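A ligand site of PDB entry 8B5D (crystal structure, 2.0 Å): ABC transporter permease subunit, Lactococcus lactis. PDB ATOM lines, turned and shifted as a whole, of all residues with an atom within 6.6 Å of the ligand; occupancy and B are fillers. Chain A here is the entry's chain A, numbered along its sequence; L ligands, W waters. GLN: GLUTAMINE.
N of the ligand sits at hydrogen-bond distance from O of Gly 68, 2.6 Å away. OD2 of Asp 9 is in hydrogen-bond range of NE2 of the ligand (2.9 Å). A nitrogen (NE2) of the ligand sits at hydrogen-bond distance from the backbone carbonyl oxygen of Ala 67 (3.0 Å). O of the ligand lies within hydrogen-bond range of N of Ala 118, 2.8 Å away. The side-chain hydroxyl (OG1) of Thr 70 is in hydrogen-bond range of a nitrogen (N) of the ligand (2.9 Å). The backbone NH (N) of Thr 70 lies within hydrogen-bond range of an oxygen (OXT) of the ligand, 2.8 Å away. The side-chain carboxylate of Asp 158 is in salt-bridge range of a nitrogen (N) of the ligand. An oxygen (OE1) of the ligand is in hydrogen-bond range of the side-chain amino group (NZ) of Lys 114. NH1 of Arg 75 lies within salt-bridge range of OXT of the ligand, at 2.7 Å.
The side-chain carboxylate (OD1) of Asp 157 lies within hydrogen-bond range of the side-chain hydroxyl (OH) of Tyr 12, at 2.9 Å. The side-chain hydroxyl of Tyr 12 lies close to the side-chain carboxylate of Asp 158 (3.2 Å). The side-chain hydroxyl (OG1) of Thr 117 lies close to the backbone NH (N) of Ala 119, 3.5 Å away. The backbone NH (N) of Arg 75 sits at hydrogen-bond distance from the side-chain hydroxyl (OG1) of Thr 72 (3.0 Å). The side-chain hydroxyl of Thr 117 sits at hydrogen-bond distance from the backbone carbonyl oxygen of Lys 114 (2.7 Å). The backbone carbonyl oxygen (O) of Gly 116 lies within hydrogen-bond range of the guanidinium group (NH2) of Arg 75. NZ of Lys 114 is in salt-bridge range of OD2 of Asp 9 (2.6 Å). The guanidinium group (NH1) of Arg 75 lies within hydrogen-bond range of the backbone carbonyl oxygen (O) of Thr 70 (2.8 Å).
Merely in contact with the ligand: Tyr 12 (3.3 Å), Phe 50 (3.5 Å), Met 69 (3.4 Å), Thr 117 (3.0 Å) and Tyr 185 (3.7 Å). Hydrophobic or aromatic side chains within 4 Å of the ligand: Tyr 12, Phe 50, Met 69, Ala 118 and Tyr 185. The nearest printed residue that does not touch the ligand is Gly 116 (4.4 Å).
Water W1 bridges the side-chain carboxylate (OD1) of Asp 157 and an oxygen (OE1) of the ligand. Water W2 bridges the side-chain carboxylate of Asp 158 and the backbone NH of Ala 119.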
ATOM      1  N   ASP A   9     -14.954  23.928  29.375  1.00  0.00           N
ATOM      2  CA  ASP A   9     -15.858  23.036  28.655  1.00  0.00           C
ATOM      3  C   ASP A   9     -16.452  21.978  29.602  1.00  0.00           C
ATOM      4  O   ASP A   9     -15.889  21.658  30.649  1.00  0.00           O
ATOM      5  CB  ASP A   9     -15.096  22.376  27.506  1.00  0.00           C
ATOM      6  CG  ASP A   9     -15.976  21.870  26.384  1.00  0.00           C
ATOM      7  OD1 ASP A   9     -17.172  21.555  26.593  1.00  0.00           O
ATOM      8  OD2 ASP A   9     -15.440  21.806  25.247  1.00  0.00           O
ATOM      9  N   SER A  11     -17.292  18.731  28.338  1.00  0.00           N
ATOM     10  CA  SER A  11     -16.800  17.410  27.948  1.00  0.00           C
ATOM     11  C   SER A  11     -15.676  17.616  26.935  1.00  0.00           C
ATOM     12  O   SER A  11     -15.928  17.820  25.753  1.00  0.00           O
ATOM     13  CB  SER A  11     -17.906  16.530  27.378  1.00  0.00           C
ATOM     14  OG  SER A  11     -17.500  15.172  27.381  1.00  0.00           O
ATOM     15  N   TYR A  12     -14.447  17.581  27.431  1.00  0.00           N
ATOM     16  CA  TYR A  12     -13.272  17.782  26.574  1.00  0.00           C
ATOM     17  C   TYR A  12     -12.076  17.014  27.150  1.00  0.00           C
ATOM     18  O   TYR A  12     -11.012  17.577  27.396  1.00  0.00           O
ATOM     19  CB  TYR A  12     -12.987  19.273  26.377  1.00  0.00           C
ATOM     20  CG  TYR A  12     -12.456  19.589  24.981  1.00  0.00           C
ATOM     21  CD1 TYR A  12     -13.097  19.116  23.832  1.00  0.00           C
ATOM     22  CD2 TYR A  12     -11.280  20.340  24.826  1.00  0.00           C
ATOM     23  CE1 TYR A  12     -12.604  19.410  22.574  1.00  0.00           C
ATOM     24  CE2 TYR A  12     -10.799  20.660  23.578  1.00  0.00           C
ATOM     25  CZ  TYR A  12     -11.440  20.176  22.456  1.00  0.00           C
ATOM     26  OH  TYR A  12     -10.908  20.486  21.225  1.00  0.00           O
ATOM     27  N   GLU A  16     -10.552  18.639  30.321  1.00  0.00           N
ATOM     28  CA  GLU A  16     -11.527  18.671  31.401  1.00  0.00           C
ATOM     29  C   GLU A  16     -12.611  17.662  31.060  1.00  0.00           C
ATOM     30  O   GLU A  16     -13.023  17.538  29.913  1.00  0.00           O
ATOM     31  CB  GLU A  16     -12.165  20.048  31.621  1.00  0.00           C
ATOM     32  CG  GLU A  16     -12.778  20.691  30.370  1.00  0.00           C
ATOM     33  CD  GLU A  16     -11.724  21.444  29.579  1.00  0.00           C
ATOM     34  OE1 GLU A  16     -10.645  21.732  30.149  1.00  0.00           O
ATOM     35  OE2 GLU A  16     -11.965  21.747  28.399  1.00  0.00           O
ATOM     36  N   GLY A  49     -19.389  24.541  29.136  1.00  0.00           N
ATOM     37  CA  GLY A  49     -19.244  24.252  27.711  1.00  0.00           C
ATOM     38  C   GLY A  49     -18.421  25.333  27.023  1.00  0.00           C
ATOM     39  O   GLY A  49     -18.289  26.426  27.586  1.00  0.00           O
ATOM     40  N   PHE A  50     -17.887  25.078  25.825  1.00  0.00           N
ATOM     41  CA  PHE A  50     -16.888  26.003  25.296  1.00  0.00           C
ATOM     42  C   PHE A  50     -17.502  27.330  24.907  1.00  0.00           C
ATOM     43  O   PHE A  50     -17.106  28.383  25.422  1.00  0.00           O
ATOM     44  CB  PHE A  50     -16.143  25.404  24.089  1.00  0.00           C
ATOM     45  CG  PHE A  50     -15.062  26.314  23.559  1.00  0.00           C
ATOM     46  CD1 PHE A  50     -13.881  26.482  24.260  1.00  0.00           C
ATOM     47  CD2 PHE A  50     -15.241  27.041  22.386  1.00  0.00           C
ATOM     48  CE1 PHE A  50     -12.884  27.317  23.802  1.00  0.00           C
ATOM     49  CE2 PHE A  50     -14.244  27.881  21.915  1.00  0.00           C
ATOM     50  CZ  PHE A  50     -13.061  28.022  22.628  1.00  0.00           C
ATOM     51  N   ALA A  67      -9.934  26.005  28.606  1.00  0.00           N
ATOM     52  CA  ALA A  67     -10.833  25.069  27.936  1.00  0.00           C
ATOM     53  C   ALA A  67     -10.221  24.503  26.656  1.00  0.00           C
ATOM     54  O   ALA A  67     -10.924  24.367  25.645  1.00  0.00           O
ATOM     55  CB  ALA A  67     -12.172  25.755  27.608  1.00  0.00           C
ATOM     56  N   GLY A  68      -8.959  24.098  26.711  1.00  0.00           N
ATOM     57  CA  GLY A  68      -8.281  23.682  25.489  1.00  0.00           C
ATOM     58  C   GLY A  68      -8.358  24.732  24.411  1.00  0.00           C
ATOM     59  O   GLY A  68      -8.481  24.399  23.222  1.00  0.00           O
ATOM     60  N   MET A  69      -8.293  26.001  24.789  1.00  0.00           N
ATOM     61  CA  MET A  69      -8.605  27.091  23.882  1.00  0.00           C
ATOM     62  C   MET A  69      -7.409  27.496  23.038  1.00  0.00           C
ATOM     63  O   MET A  69      -6.371  27.903  23.588  1.00  0.00           O
ATOM     64  CB  MET A  69      -9.096  28.298  24.668  1.00  0.00           C
ATOM     65  CG  MET A  69      -9.926  29.228  23.830  1.00  0.00           C
ATOM     66  SD  MET A  69     -10.524  30.515  24.904  1.00  0.00           S
ATOM     67  CE  MET A  69     -10.700  31.868  23.716  1.00  0.00           C
ATOM     68  N   THR A  70      -7.576  27.432  21.722  1.00  0.00           N
ATOM     69  CA  THR A  70      -6.513  27.758  20.798  1.00  0.00           C
ATOM     70  C   THR A  70      -6.299  29.258  20.714  1.00  0.00           C
ATOM     71  O   THR A  70      -7.253  30.023  20.539  1.00  0.00           O
ATOM     72  CB  THR A  70      -6.835  27.193  19.417  1.00  0.00           C
ATOM     73  OG1 THR A  70      -7.068  25.796  19.543  1.00  0.00           O
ATOM     74  CG2 THR A  70      -5.642  27.416  18.454  1.00  0.00           C
ATOM     75  N   ILE A  71      -5.039  29.650  20.823  1.00  0.00           N
ATOM     76  CA  ILE A  71      -4.614  31.035  20.600  1.00  0.00           C
ATOM     77  C   ILE A  71      -4.598  31.278  19.096  1.00  0.00           C
ATOM     78  O   ILE A  71      -3.921  30.558  18.361  1.00  0.00           O
ATOM     79  CB  ILE A  71      -3.231  31.303  21.211  1.00  0.00           C
ATOM     80  CG1 ILE A  71      -3.204  31.036  22.727  1.00  0.00           C
ATOM     81  CG2 ILE A  71      -2.768  32.712  20.860  1.00  0.00           C
ATOM     82  CD1 ILE A  71      -1.826  31.128  23.337  1.00  0.00           C
ATOM     83  N   THR A  72      -5.324  32.288  18.653  1.00  0.00           N
ATOM     84  CA  THR A  72      -5.322  32.672  17.252  1.00  0.00           C
ATOM     85  C   THR A  72      -5.260  34.188  17.134  1.00  0.00           C
ATOM     86  O   THR A  72      -5.655  34.904  18.054  1.00  0.00           O
ATOM     87  CB  THR A  72      -6.559  32.133  16.511  1.00  0.00           C
ATOM     88  OG1 THR A  72      -7.687  32.941  16.833  1.00  0.00           O
ATOM     89  CG2 THR A  72      -6.836  30.664  16.861  1.00  0.00           C
ATOM     90  N   ARG A  75      -8.638  35.775  17.391  1.00  0.00           N
ATOM     91  CA  ARG A  75      -9.163  35.724  18.740  1.00  0.00           C
ATOM     92  C   ARG A  75      -8.442  36.745  19.595  1.00  0.00           C
ATOM     93  O   ARG A  75      -9.033  37.297  20.557  1.00  0.00           O
ATOM     94  CB  ARG A  75      -8.954  34.323  19.298  1.00  0.00           C
ATOM     95  CG  ARG A  75     -10.105  33.399  18.940  1.00  0.00           C
ATOM     96  CD  ARG A  75      -9.786  32.010  19.376  1.00  0.00           C
ATOM     97  NE  ARG A  75     -10.944  31.165  19.257  1.00  0.00           N
ATOM     98  CZ  ARG A  75     -10.967  29.889  19.622  1.00  0.00           C
ATOM     99  NH1 ARG A  75      -9.867  29.289  20.047  1.00  0.00           N
ATOM    100  NH2 ARG A  75     -12.099  29.196  19.494  1.00  0.00           N
ATOM    101  N   SER A  88      -1.696  22.833  19.518  1.00  0.00           N
ATOM    102  CA  SER A  88      -3.052  22.931  18.992  1.00  0.00           C
ATOM    103  C   SER A  88      -3.072  22.360  17.582  1.00  0.00           C
ATOM    104  O   SER A  88      -2.442  22.915  16.675  1.00  0.00           O
ATOM    105  CB  SER A  88      -3.526  24.382  18.991  1.00  0.00           C
ATOM    106  OG  SER A  88      -2.562  25.256  18.428  1.00  0.00           O
ATOM    107  N   LEU A  90      -5.860  20.177  14.654  1.00  0.00           N
ATOM    108  CA  LEU A  90      -7.200  19.784  14.227  1.00  0.00           C
ATOM    109  C   LEU A  90      -7.101  18.567  13.323  1.00  0.00           C
ATOM    110  O   LEU A  90      -6.134  18.414  12.576  1.00  0.00           O
ATOM    111  CB  LEU A  90      -7.887  20.912  13.464  1.00  0.00           C
ATOM    112  CG  LEU A  90      -8.068  22.242  14.166  1.00  0.00           C
ATOM    113  CD1 LEU A  90      -8.646  23.275  13.207  1.00  0.00           C
ATOM    114  CD2 LEU A  90      -8.963  22.063  15.371  1.00  0.00           C
ATOM    115  N   LYS A 114     -18.002  22.097  16.663  1.00  0.00           N
ATOM    116  CA  LYS A 114     -18.594  22.772  17.811  1.00  0.00           C
ATOM    117  C   LYS A 114     -18.601  24.278  17.608  1.00  0.00           C
ATOM    118  O   LYS A 114     -17.701  24.852  16.996  1.00  0.00           O
ATOM    119  CB  LYS A 114     -17.866  22.411  19.110  1.00  0.00           C
ATOM    120  CG  LYS A 114     -17.942  20.942  19.468  1.00  0.00           C
ATOM    121  CD  LYS A 114     -16.838  20.535  20.474  1.00  0.00           C
ATOM    122  CE  LYS A 114     -16.790  21.463  21.691  1.00  0.00           C
ATOM    123  NZ  LYS A 114     -15.856  20.926  22.790  1.00  0.00           N
ATOM    124  N   GLY A 116     -18.253  28.159  17.705  1.00  0.00           N
ATOM    125  CA  GLY A 116     -17.284  29.097  18.235  1.00  0.00           C
ATOM    126  C   GLY A 116     -15.854  28.613  18.276  1.00  0.00           C
ATOM    127  O   GLY A 116     -14.996  29.344  18.780  1.00  0.00           O
ATOM    128  N   THR A 117     -15.566  27.427  17.735  1.00  0.00           N
ATOM    129  CA  THR A 117     -14.271  26.783  17.914  1.00  0.00           C
ATOM    130  C   THR A 117     -13.328  26.983  16.723  1.00  0.00           C
ATOM    131  O   THR A 117     -13.715  27.464  15.658  1.00  0.00           O
ATOM    132  CB  THR A 117     -14.445  25.285  18.150  1.00  0.00           C
ATOM    133  OG1 THR A 117     -14.994  24.682  16.983  1.00  0.00           O
ATOM    134  CG2 THR A 117     -15.322  25.020  19.381  1.00  0.00           C
ATOM    135  N   ALA A 118     -12.041  26.643  16.925  1.00  0.00           N
ATOM    136  CA  ALA A 118     -11.080  26.655  15.826  1.00  0.00           C
ATOM    137  C   ALA A 118     -11.493  25.665  14.719  1.00  0.00           C
ATOM    138  O   ALA A 118     -11.279  25.933  13.538  1.00  0.00           O
ATOM    139  CB  ALA A 118      -9.657  26.366  16.349  1.00  0.00           C
ATOM    140  N   ALA A 119     -12.103  24.543  15.085  1.00  0.00           N
ATOM    141  CA  ALA A 119     -12.591  23.607  14.072  1.00  0.00           C
ATOM    142  C   ALA A 119     -13.638  24.274  13.176  1.00  0.00           C
ATOM    143  O   ALA A 119     -13.518  24.258  11.937  1.00  0.00           O
ATOM    144  CB  ALA A 119     -13.180  22.370  14.726  1.00  0.00           C
ATOM    145  N   ASP A 157     -12.322  18.164  15.169  1.00  0.00           N
ATOM    146  CA  ASP A 157     -12.051  18.517  16.551  1.00  0.00           C
ATOM    147  C   ASP A 157     -10.542  18.385  16.760  1.00  0.00           C
ATOM    148  O   ASP A 157      -9.807  18.010  15.849  1.00  0.00           O
ATOM    149  CB  ASP A 157     -12.894  17.652  17.494  1.00  0.00           C
ATOM    150  CG  ASP A 157     -13.153  18.310  18.836  1.00  0.00           C
ATOM    151  OD1 ASP A 157     -12.611  19.418  19.115  1.00  0.00           O
ATOM    152  OD2 ASP A 157     -13.930  17.709  19.616  1.00  0.00           O
ATOM    153  N   ASP A 158     -10.085  18.671  17.971  1.00  0.00           N
ATOM    154  CA  ASP A 158      -8.651  18.698  18.208  1.00  0.00           C
ATOM    155  C   ASP A 158      -8.090  17.290  18.369  1.00  0.00           C
ATOM    156  O   ASP A 158      -8.738  16.375  18.895  1.00  0.00           O
ATOM    157  CB  ASP A 158      -8.334  19.540  19.450  1.00  0.00           C
ATOM    158  CG  ASP A 158      -8.677  20.987  19.259  1.00  0.00           C
ATOM    159  OD1 ASP A 158      -9.581  21.302  18.452  1.00  0.00           O
ATOM    160  OD2 ASP A 158      -8.060  21.821  19.929  1.00  0.00           O
ATOM    161  N   TYR A 185      -2.592  26.098  22.862  1.00  0.00           N
ATOM    162  CA  TYR A 185      -3.660  26.381  23.833  1.00  0.00           C
ATOM    163  C   TYR A 185      -3.209  27.392  24.878  1.00  0.00           C
ATOM    164  O   TYR A 185      -2.112  27.269  25.427  1.00  0.00           O
ATOM    165  CB  TYR A 185      -4.095  25.116  24.569  1.00  0.00           C
ATOM    166  CG  TYR A 185      -4.761  24.036  23.742  1.00  0.00           C
ATOM    167  CD1 TYR A 185      -5.187  24.272  22.442  1.00  0.00           C
ATOM    168  CD2 TYR A 185      -4.966  22.774  24.279  1.00  0.00           C
ATOM    169  CE1 TYR A 185      -5.788  23.259  21.708  1.00  0.00           C
ATOM    170  CE2 TYR A 185      -5.568  21.765  23.554  1.00  0.00           C
ATOM    171  CZ  TYR A 185      -5.974  22.005  22.286  1.00  0.00           C
ATOM    172  OH  TYR A 185      -6.575  20.985  21.587  1.00  0.00           O
HETATM  173  N   GLN L   1      -9.222  24.223  20.771  1.00  0.00           N
HETATM  174  CA  GLN L   1     -10.523  24.496  20.107  1.00  0.00           C
HETATM  175  C   GLN L   1     -10.851  25.990  20.201  1.00  0.00           C
HETATM  176  O   GLN L   1     -11.835  26.424  19.666  1.00  0.00           O
HETATM  177  CB  GLN L   1     -11.599  23.637  20.756  1.00  0.00           C
HETATM  178  CG  GLN L   1     -11.888  23.980  22.209  1.00  0.00           C
HETATM  179  CD  GLN L   1     -13.026  23.149  22.758  1.00  0.00           C
HETATM  180  OE1 GLN L   1     -13.806  22.543  22.018  1.00  0.00           O
HETATM  181  NE2 GLN L   1     -13.109  23.091  24.072  1.00  0.00           N
HETATM  182  OXT GLN L   1     -10.079  26.677  20.852  1.00  0.00           O
HETATM  183  O   HOH W   1     -13.645  21.614  19.245  1.00  0.00           O
HETATM  184  O   HOH W   2     -11.531  22.835  17.480  1.00  0.00           O
